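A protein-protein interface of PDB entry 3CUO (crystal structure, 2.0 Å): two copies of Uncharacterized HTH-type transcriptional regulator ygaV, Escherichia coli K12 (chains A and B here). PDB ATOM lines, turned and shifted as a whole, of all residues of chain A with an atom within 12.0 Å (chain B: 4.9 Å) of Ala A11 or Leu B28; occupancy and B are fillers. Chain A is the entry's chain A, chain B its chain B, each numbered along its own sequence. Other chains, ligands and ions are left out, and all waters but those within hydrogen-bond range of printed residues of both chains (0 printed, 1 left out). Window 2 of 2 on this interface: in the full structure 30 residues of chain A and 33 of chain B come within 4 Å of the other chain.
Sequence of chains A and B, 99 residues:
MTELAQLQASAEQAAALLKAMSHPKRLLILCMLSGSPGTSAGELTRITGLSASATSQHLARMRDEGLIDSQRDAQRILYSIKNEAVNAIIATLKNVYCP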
ATOM      1  N   MET A   1     -21.768  17.944  36.738  1.00  0.00           N
ATOM      2  CA  MET A   1     -22.450  18.839  35.704  1.00  0.00           C
ATOM      3  C   MET A   1     -21.583  20.072  35.320  1.00  0.00           C
ATOM      4  O   MET A   1     -21.399  20.373  34.132  1.00  0.00           O
ATOM      5  CB  MET A   1     -23.864  19.243  36.151  1.00  0.00           C
ATOM      6  CG  MET A   1     -24.832  19.728  35.037  1.00  0.00           C
ATOM      7  SD  MET A   1     -24.964  18.808  33.455  1.00  0.00           S
ATOM      8  CE  MET A   1     -23.898  19.792  32.411  1.00  0.00           C
ATOM      9  N   THR A   2     -20.988  20.718  36.318  1.00  0.00           N
ATOM     10  CA  THR A   2     -20.008  21.774  36.083  1.00  0.00           C
ATOM     11  C   THR A   2     -18.763  21.249  35.401  1.00  0.00           C
ATOM     12  O   THR A   2     -18.227  21.922  34.493  1.00  0.00           O
ATOM     13  CB  THR A   2     -19.590  22.454  37.388  1.00  0.00           C
ATOM     14  OG1 THR A   2     -20.748  22.998  38.002  1.00  0.00           O
ATOM     15  CG2 THR A   2     -18.593  23.570  37.143  1.00  0.00           C
ATOM     16  N   GLU A   3     -18.272  20.070  35.825  1.00  0.00           N
ATOM     17  CA  GLU A   3     -17.114  19.500  35.167  1.00  0.00           C
ATOM     18  C   GLU A   3     -17.466  19.207  33.731  1.00  0.00           C
ATOM     19  O   GLU A   3     -16.654  19.395  32.819  1.00  0.00           O
ATOM     20  CB  GLU A   3     -16.646  18.176  35.810  1.00  0.00           C
ATOM     21  CG  GLU A   3     -15.795  18.323  37.028  1.00  0.00           C
ATOM     22  CD  GLU A   3     -16.542  18.885  38.244  1.00  0.00           C
ATOM     23  OE1 GLU A   3     -17.775  18.730  38.381  1.00  0.00           O
ATOM     24  OE2 GLU A   3     -15.850  19.463  39.101  1.00  0.00           O
ATOM     25  N   LEU A   4     -18.668  18.677  33.537  1.00  0.00           N
ATOM     26  CA  LEU A   4     -19.118  18.337  32.210  1.00  0.00           C
ATOM     27  C   LEU A   4     -19.168  19.598  31.342  1.00  0.00           C
ATOM     28  O   LEU A   4     -18.712  19.583  30.191  1.00  0.00           O
ATOM     29  CB  LEU A   4     -20.488  17.658  32.274  1.00  0.00           C
ATOM     30  CG  LEU A   4     -21.002  17.245  30.905  1.00  0.00           C
ATOM     31  CD1 LEU A   4     -20.070  16.262  30.319  1.00  0.00           C
ATOM     32  CD2 LEU A   4     -22.420  16.690  30.941  1.00  0.00           C
ATOM     33  N   ALA A   5     -19.744  20.677  31.877  1.00  0.00           N
ATOM     34  CA  ALA A   5     -19.902  21.923  31.133  1.00  0.00           C
ATOM     35  C   ALA A   5     -18.525  22.568  30.780  1.00  0.00           C
ATOM     36  O   ALA A   5     -18.318  23.130  29.686  1.00  0.00           O
ATOM     37  CB  ALA A   5     -20.801  22.871  31.928  1.00  0.00           C
ATOM     38  N   GLN A   6     -17.533  22.427  31.657  1.00  0.00           N
ATOM     39  CA  GLN A   6     -16.236  23.052  31.373  1.00  0.00           C
ATOM     40  C   GLN A   6     -15.446  22.266  30.352  1.00  0.00           C
ATOM     41  O   GLN A   6     -14.756  22.858  29.511  1.00  0.00           O
ATOM     42  CB  GLN A   6     -15.423  23.154  32.637  1.00  0.00           C
ATOM     43  CG  GLN A   6     -15.994  24.119  33.670  1.00  0.00           C
ATOM     44  CD  GLN A   6     -15.287  23.916  35.003  1.00  0.00           C
ATOM     45  OE1 GLN A   6     -15.492  22.897  35.701  1.00  0.00           O
ATOM     46  NE2 GLN A   6     -14.415  24.871  35.348  1.00  0.00           N
ATOM     47  N   LEU A   7     -15.570  20.939  30.376  1.00  0.00           N
ATOM     48  CA  LEU A   7     -14.704  20.154  29.588  1.00  0.00           C
ATOM     49  C   LEU A   7     -15.318  19.576  28.362  1.00  0.00           C
ATOM     50  O   LEU A   7     -14.599  19.015  27.532  1.00  0.00           O
ATOM     51  CB  LEU A   7     -14.150  18.993  30.482  1.00  0.00           C
ATOM     52  CG  LEU A   7     -12.782  18.423  30.238  1.00  0.00           C
ATOM     53  CD1 LEU A   7     -11.784  19.535  30.215  1.00  0.00           C
ATOM     54  CD2 LEU A   7     -12.517  17.347  31.347  1.00  0.00           C
ATOM     55  N   GLN A   8     -16.636  19.594  28.223  1.00  0.00           N
ATOM     56  CA  GLN A   8     -17.201  18.780  27.156  1.00  0.00           C
ATOM     57  C   GLN A   8     -16.794  19.218  25.771  1.00  0.00           C
ATOM     58  O   GLN A   8     -16.558  18.378  24.898  1.00  0.00           O
ATOM     59  CB  GLN A   8     -18.737  18.655  27.252  1.00  0.00           C
ATOM     60  CG  GLN A   8     -19.521  19.933  27.089  1.00  0.00           C
ATOM     61  CD  GLN A   8     -21.016  19.679  27.357  1.00  0.00           C
ATOM     62  OE1 GLN A   8     -21.444  18.525  27.458  1.00  0.00           O
ATOM     63  NE2 GLN A   8     -21.803  20.749  27.442  1.00  0.00           N
ATOM     64  N   ALA A   9     -16.695  20.527  25.548  1.00  0.00           N
ATOM     65  CA  ALA A   9     -16.231  21.030  24.238  1.00  0.00           C
ATOM     66  C   ALA A   9     -14.786  20.660  23.945  1.00  0.00           C
ATOM     67  O   ALA A   9     -14.347  20.802  22.820  1.00  0.00           O
ATOM     68  CB  ALA A   9     -16.393  22.520  24.179  1.00  0.00           C
ATOM     69  N   SER A  10     -14.056  20.171  24.953  1.00  0.00           N
ATOM     70  CA  SER A  10     -12.629  19.814  24.846  1.00  0.00           C
ATOM     71  C   SER A  10     -12.356  18.328  24.956  1.00  0.00           C
ATOM     72  O   SER A  10     -11.165  17.876  24.985  1.00  0.00           O
ATOM     73  CB  SER A  10     -11.872  20.468  26.004  1.00  0.00           C
ATOM     74  OG  SER A  10     -11.724  21.828  25.784  1.00  0.00           O
ATOM     75  N   ALA A  11     -13.429  17.563  25.071  1.00  0.00           N
ATOM     76  CA  ALA A  11     -13.315  16.145  25.439  1.00  0.00           C
ATOM     77  C   ALA A  11     -12.622  15.353  24.338  1.00  0.00           C
ATOM     78  O   ALA A  11     -11.932  14.432  24.605  1.00  0.00           O
ATOM     79  CB  ALA A  11     -14.686  15.581  25.762  1.00  0.00           C
ATOM     80  N   GLU A  12     -12.743  15.784  23.082  1.00  0.00           N
ATOM     81  CA  GLU A  12     -12.150  15.030  22.007  1.00  0.00           C
ATOM     82  C   GLU A  12     -10.625  15.310  21.998  1.00  0.00           C
ATOM     83  O   GLU A  12      -9.804  14.405  21.805  1.00  0.00           O
ATOM     84  CB  GLU A  12     -12.830  15.375  20.646  1.00  0.00           C
ATOM     85  CG  GLU A  12     -14.278  14.886  20.585  1.00  0.00           C
ATOM     86  CD  GLU A  12     -14.896  14.925  19.193  1.00  0.00           C
ATOM     87  OE1 GLU A  12     -14.522  15.801  18.366  1.00  0.00           O
ATOM     88  OE2 GLU A  12     -15.774  14.070  18.929  1.00  0.00           O
ATOM     89  N   GLN A  13     -10.247  16.550  22.266  1.00  0.00           N
ATOM     90  CA  GLN A  13      -8.842  16.843  22.349  1.00  0.00           C
ATOM     91  C   GLN A  13      -8.203  16.290  23.643  1.00  0.00           C
ATOM     92  O   GLN A  13      -7.079  15.829  23.619  1.00  0.00           O
ATOM     93  CB  GLN A  13      -8.526  18.335  22.150  1.00  0.00           C
ATOM     94  CG  GLN A  13      -9.375  19.334  22.904  1.00  0.00           C
ATOM     95  CD  GLN A  13      -9.275  20.744  22.275  1.00  0.00           C
ATOM     96  OE1 GLN A  13      -8.148  21.251  22.042  1.00  0.00           O
ATOM     97  NE2 GLN A  13     -10.452  21.365  21.954  1.00  0.00           N
ATOM     98  N   ALA A  14      -8.915  16.416  24.758  1.00  0.00           N
ATOM     99  CA  ALA A  14      -8.503  15.835  26.010  1.00  0.00           C
ATOM    100  C   ALA A  14      -8.257  14.306  25.868  1.00  0.00           C
ATOM    101  O   ALA A  14      -7.259  13.850  26.315  1.00  0.00           O
ATOM    102  CB  ALA A  14      -9.545  16.175  27.115  1.00  0.00           C
ATOM    103  N   ALA A  15      -9.197  13.544  25.295  1.00  0.00           N
ATOM    104  CA  ALA A  15      -9.061  12.123  25.050  1.00  0.00           C
ATOM    105  C   ALA A  15      -7.869  11.750  24.186  1.00  0.00           C
ATOM    106  O   ALA A  15      -7.191  10.712  24.406  1.00  0.00           O
ATOM    107  CB  ALA A  15     -10.364  11.530  24.441  1.00  0.00           C
ATOM    108  N   ALA A  16      -7.662  12.538  23.143  1.00  0.00           N
ATOM    109  CA  ALA A  16      -6.527  12.419  22.253  1.00  0.00           C
ATOM    110  C   ALA A  16      -5.175  12.613  22.962  1.00  0.00           C
ATOM    111  O   ALA A  16      -4.234  11.891  22.714  1.00  0.00           O
ATOM    112  CB  ALA A  16      -6.644  13.480  21.133  1.00  0.00           C
ATOM    113  N   LEU A  17      -5.084  13.636  23.805  1.00  0.00           N
ATOM    114  CA  LEU A  17      -3.925  13.846  24.620  1.00  0.00           C
ATOM    115  C   LEU A  17      -3.662  12.637  25.533  1.00  0.00           C
ATOM    116  O   LEU A  17      -2.559  12.127  25.583  1.00  0.00           O
ATOM    117  CB  LEU A  17      -4.100  15.089  25.431  1.00  0.00           C
ATOM    118  CG  LEU A  17      -2.938  15.426  26.354  1.00  0.00           C
ATOM    119  CD1 LEU A  17      -1.854  16.139  25.571  1.00  0.00           C
ATOM    120  CD2 LEU A  17      -3.450  16.263  27.520  1.00  0.00           C
ATOM    121  N   LEU A  18      -4.682  12.145  26.240  1.00  0.00           N
ATOM    122  CA  LEU A  18      -4.500  11.026  27.117  1.00  0.00           C
ATOM    123  C   LEU A  18      -4.111   9.794  26.315  1.00  0.00           C
ATOM    124  O   LEU A  18      -3.242   9.010  26.685  1.00  0.00           O
ATOM    125  CB  LEU A  18      -5.800  10.803  27.962  1.00  0.00           C
ATOM    126  CG  LEU A  18      -6.250  11.852  28.974  1.00  0.00           C
ATOM    127  CD1 LEU A  18      -7.355  11.208  29.813  1.00  0.00           C
ATOM    128  CD2 LEU A  18      -5.101  12.389  29.852  1.00  0.00           C
ATOM    129  N   LYS A  19      -4.718   9.624  25.170  1.00  0.00           N
ATOM    130  CA  LYS A  19      -4.392   8.449  24.363  1.00  0.00           C
ATOM    131  C   LYS A  19      -2.947   8.450  23.890  1.00  0.00           C
ATOM    132  O   LYS A  19      -2.289   7.396  23.924  1.00  0.00           O
ATOM    133  CB  LYS A  19      -5.354   8.353  23.202  1.00  0.00           C
ATOM    134  CG  LYS A  19      -5.067   7.182  22.260  1.00  0.00           C
ATOM    135  CD  LYS A  19      -6.358   6.748  21.559  1.00  0.00           C
ATOM    136  CE  LYS A  19      -6.093   6.208  20.130  1.00  0.00           C
ATOM    137  NZ  LYS A  19      -6.889   4.921  19.839  1.00  0.00           N
ATOM    138  N   ALA A  20      -2.425   9.635  23.490  1.00  0.00           N
ATOM    139  CA  ALA A  20      -1.037   9.730  23.097  1.00  0.00           C
ATOM    140  C   ALA A  20      -0.023   9.457  24.215  1.00  0.00           C
ATOM    141  O   ALA A  20       1.131   9.119  23.951  1.00  0.00           O
ATOM    142  CB  ALA A  20      -0.746  11.163  22.436  1.00  0.00           C
ATOM    143  N   GLU A  65       1.414  14.239  17.393  1.00  0.00           N
ATOM    144  CA  GLU A  65       0.303  14.483  18.286  1.00  0.00           C
ATOM    145  C   GLU A  65       0.410  15.778  19.136  1.00  0.00           C
ATOM    146  O   GLU A  65      -0.507  16.109  19.918  1.00  0.00           O
ATOM    147  CB  GLU A  65       0.147  13.240  19.198  1.00  0.00           C
ATOM    148  CG  GLU A  65      -0.632  12.136  18.544  1.00  0.00           C
ATOM    149  CD  GLU A  65      -2.077  12.543  18.285  1.00  0.00           C
ATOM    150  OE1 GLU A  65      -2.834  12.782  19.256  1.00  0.00           O
ATOM    151  OE2 GLU A  65      -2.454  12.688  17.102  1.00  0.00           O
ATOM    152  N   ILE A  89       0.002  16.770  33.428  1.00  0.00           N
ATOM    153  CA  ILE A  89      -0.457  15.406  33.645  1.00  0.00           C
ATOM    154  C   ILE A  89       0.612  14.607  34.349  1.00  0.00           C
ATOM    155  O   ILE A  89       0.335  13.861  35.301  1.00  0.00           O
ATOM    156  CB  ILE A  89      -0.891  14.793  32.330  1.00  0.00           C
ATOM    157  CG1 ILE A  89      -2.152  15.515  31.899  1.00  0.00           C
ATOM    158  CG2 ILE A  89      -1.055  13.213  32.439  1.00  0.00           C
ATOM    159  CD1 ILE A  89      -2.440  15.449  30.484  1.00  0.00           C
ATOM    160  N   PRO B  24     -13.509  10.164  24.467  1.00  0.00           N
ATOM    161  CA  PRO B  24     -14.221  11.355  24.828  1.00  0.00           C
ATOM    162  C   PRO B  24     -15.523  11.087  25.588  1.00  0.00           C
ATOM    163  O   PRO B  24     -15.881  11.851  26.481  1.00  0.00           O
ATOM    164  CB  PRO B  24     -14.472  12.064  23.458  1.00  0.00           C
ATOM    165  CG  PRO B  24     -14.361  11.002  22.460  1.00  0.00           C
ATOM    166  CD  PRO B  24     -13.370  10.029  23.004  1.00  0.00           C
ATOM    167  N   LYS B  25     -16.248  10.051  25.229  1.00  0.00           N
ATOM    168  CA  LYS B  25     -17.541   9.750  25.919  1.00  0.00           C
ATOM    169  C   LYS B  25     -17.312   9.189  27.338  1.00  0.00           C
ATOM    170  O   LYS B  25     -18.025   9.551  28.236  1.00  0.00           O
ATOM    171  CB  LYS B  25     -18.453   8.837  25.100  1.00  0.00           C
ATOM    172  CG  LYS B  25     -18.936   9.411  23.728  1.00  0.00           C
ATOM    173  CD  LYS B  25     -19.563  10.821  23.795  1.00  0.00           C
ATOM    174  CE  LYS B  25     -20.149  11.275  22.422  1.00  0.00           C
ATOM    175  NZ  LYS B  25     -20.479  12.712  22.522  1.00  0.00           N
ATOM    176  N   ARG B  26     -16.251   8.432  27.549  1.00  0.00           N
ATOM    177  CA  ARG B  26     -15.801   8.080  28.921  1.00  0.00           C
ATOM    178  C   ARG B  26     -15.387   9.313  29.730  1.00  0.00           C
ATOM    179  O   ARG B  26     -15.809   9.450  30.865  1.00  0.00           O
ATOM    180  CB  ARG B  26     -14.659   7.127  28.883  1.00  0.00           C
ATOM    181  CG  ARG B  26     -15.021   5.811  28.373  1.00  0.00           C
ATOM    182  CD  ARG B  26     -13.949   4.907  28.579  1.00  0.00           C
ATOM    183  NE  ARG B  26     -14.371   3.603  28.106  1.00  0.00           N
ATOM    184  CZ  ARG B  26     -13.674   2.490  28.242  1.00  0.00           C
ATOM    185  NH1 ARG B  26     -12.504   2.462  28.894  1.00  0.00           N
ATOM    186  NH2 ARG B  26     -14.182   1.373  27.729  1.00  0.00           N
ATOM    187  N   LEU B  27     -14.707  10.290  29.125  1.00  0.00           N
ATOM    188  CA  LEU B  27     -14.518  11.571  29.829  1.00  0.00           C
ATOM    189  C   LEU B  27     -15.756  12.269  30.179  1.00  0.00           C
ATOM    190  O   LEU B  27     -15.805  12.882  31.239  1.00  0.00           O
ATOM    191  CB  LEU B  27     -13.581  12.598  29.092  1.00  0.00           C
ATOM    192  CG  LEU B  27     -12.174  12.110  28.959  1.00  0.00           C
ATOM    193  CD1 LEU B  27     -11.360  13.197  28.138  1.00  0.00           C
ATOM    194  CD2 LEU B  27     -11.536  11.816  30.360  1.00  0.00           C
ATOM    195  N   LEU B  28     -16.785  12.266  29.328  1.00  0.00           N
ATOM    196  CA  LEU B  28     -17.954  12.958  29.694  1.00  0.00           C
ATOM    197  C   LEU B  28     -18.569  12.262  30.913  1.00  0.00           C
ATOM    198  O   LEU B  28     -19.162  12.871  31.848  1.00  0.00           O
ATOM    199  CB  LEU B  28     -18.979  12.960  28.541  1.00  0.00           C
ATOM    200  CG  LEU B  28     -18.994  14.065  27.475  1.00  0.00           C
ATOM    201  CD1 LEU B  28     -17.725  14.728  27.301  1.00  0.00           C
ATOM    202  CD2 LEU B  28     -19.539  13.427  26.184  1.00  0.00           C
ATOM    203  N   ILE B  29     -18.593  10.971  30.809  1.00  0.00           N
ATOM    204  CA  ILE B  29     -19.220  10.172  31.891  1.00  0.00           C
ATOM    205  C   ILE B  29     -18.398  10.372  33.187  1.00  0.00           C
ATOM    206  O   ILE B  29     -18.955  10.549  34.236  1.00  0.00           O
ATOM    207  CB  ILE B  29     -19.217   8.710  31.569  1.00  0.00           C
ATOM    208  CG1 ILE B  29     -20.162   8.332  30.426  1.00  0.00           C
ATOM    209  CG2 ILE B  29     -19.538   7.879  32.854  1.00  0.00           C
ATOM    210  CD1 ILE B  29     -20.018   6.879  29.961  1.00  0.00           C
ATOM    211  N   LEU B  30     -17.076  10.262  33.103  1.00  0.00           N
ATOM    212  CA  LEU B  30     -16.242  10.470  34.293  1.00  0.00           C
ATOM    213  C   LEU B  30     -16.421  11.901  34.846  1.00  0.00           C
ATOM    214  O   LEU B  30     -16.478  12.071  36.047  1.00  0.00           O
ATOM    215  CB  LEU B  30     -14.786  10.051  34.067  1.00  0.00           C
ATOM    216  CG  LEU B  30     -14.608   8.555  33.774  1.00  0.00           C
ATOM    217  CD1 LEU B  30     -13.180   8.187  33.252  1.00  0.00           C
ATOM    218  CD2 LEU B  30     -15.011   7.684  34.996  1.00  0.00           C
ATOM    219  N   CYS B  31     -16.584  12.914  33.981  1.00  0.00           N
ATOM    220  CA  CYS B  31     -16.847  14.274  34.441  1.00  0.00           C
ATOM    221  C   CYS B  31     -18.150  14.402  35.185  1.00  0.00           C
ATOM    222  O   CYS B  31     -18.248  15.018  36.274  1.00  0.00           O
ATOM    223  CB  CYS B  31     -16.920  15.261  33.260  1.00  0.00           C
ATOM    224  SG  CYS B  31     -15.466  15.836  32.621  1.00  0.00           S
ATOM    225  N   MET B  32     -19.216  13.849  34.598  1.00  0.00           N
ATOM    226  CA  MET B  32     -20.505  13.837  35.306  1.00  0.00           C
ATOM    227  C   MET B  32     -20.465  13.059  36.630  1.00  0.00           C
ATOM    228  O   MET B  32     -21.069  13.463  37.619  1.00  0.00           O
ATOM    229  CB  MET B  32     -21.608  13.248  34.404  1.00  0.00           C
ATOM    230  CG  MET B  32     -23.028  13.429  34.935  1.00  0.00           C
ATOM    231  SD  MET B  32     -23.613  15.139  34.694  1.00  0.00           S
ATOM    232  CE  MET B  32     -24.814  15.016  35.943  1.00  0.00           C
ATOM    233  N   ILE B  47     -26.624  12.725  28.877  1.00  0.00           N
ATOM    234  CA  ILE B  47     -25.438  13.629  28.731  1.00  0.00           C
ATOM    235  C   ILE B  47     -24.413  13.264  27.657  1.00  0.00           C
ATOM    236  O   ILE B  47     -23.675  14.123  27.159  1.00  0.00           O
ATOM    237  CB  ILE B  47     -24.754  13.971  30.119  1.00  0.00           C
ATOM    238  CG1 ILE B  47     -23.923  12.798  30.701  1.00  0.00           C
ATOM    239  CG2 ILE B  47     -25.874  14.456  31.141  1.00  0.00           C
ATOM    240  CD1 ILE B  47     -22.478  12.651  30.149  1.00  0.00           C
ATOM    241  N   THR B  48     -24.327  12.005  27.277  1.00  0.00           N
ATOM    242  CA  THR B  48     -23.324  11.621  26.287  1.00  0.00           C
ATOM    243  C   THR B  48     -23.915  11.587  24.891  1.00  0.00           C
ATOM    244  O   THR B  48     -23.161  11.545  23.910  1.00  0.00           O
ATOM    245  CB  THR B  48     -22.743  10.233  26.548  1.00  0.00           C
ATOM    246  OG1 THR B  48     -23.796   9.268  26.428  1.00  0.00           O
ATOM    247  CG2 THR B  48     -22.056  10.170  27.919  1.00  0.00           C
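Met A1 touches Met B32 (N to SD, 3.9 Å). Leu B28 touches Leu A4. CB of Cys B31 touches N of Leu A4 (3.8 Å). Ile B47 touches Leu A4 (CB to CD2, 3.7 Å). Leu A7 touches Cys B31 (CD2 to SG, 3.6 Å). Pro B24 touches Ala A11. Ala A11 touches Leu B27 (O to CD1, 3.8 Å). Ala A11 touches Leu B28. Ala A14 touches Leu B27 (CB to CD1, 3.6 Å). CD1 of Leu B27 touches N of Ala A15, 3.6 Å away.
No position is printed for both chains.
Printed residues of chain B within 4 Å of Ala A11: Pro B24 (3.7 Å), Leu B27 (3.8 Å) and Leu B28 (3.5 Å). Of chain A, only Leu A4 (3.8 Å) and Ala A11 (3.5 Å) come within 4 Å of Leu B28. Pro B24 touches two residues of chain A. No residue of chain A comes within 4 Å of Lys B25. No residue of chain A comes within 4 Å of Leu B30. Printed residues of chain B within 4 Å of Leu A4: Leu B28, Cys B31 and Ile B47. Of the printed residues of chain B, Met A1 touches Met B32 (3.9 Å). Of the printed residues of chain B, Glu A3 touches Cys B31 (3.6 Å). Of the printed residues of chain B, Ala A15 touches Pro B24 and Leu B27. Of the printed residues of chain B, Ala A14 touches Leu B27.
Of the 22 printed residues of chain A, 7 touch a printed residue of chain B. Hydrophobic or aromatic side chains of chain A that line the printed part of chain B: Leu A4, Leu A7, Ala A11, Ala A14 and Ala A15. Along chain B the printed residues that touch a printed residue of chain A span positions 24 to 47. Among the printed residues, no Asp or Glu carboxylate lies within 4 Å of a Lys or Arg side-chain nitrogen of the other chain.
The backbone carbonyl oxygen (O) of Leu B27 is in hydrogen-bond range of the side-chain sulfur (SG) of Cys B31 (3.3 Å).
The backbone carbonyl oxygen (O) of Glu A3 sits at hydrogen-bond distance from the side-chain sulfur (SG) of Cys B31, at 3.8 Å.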
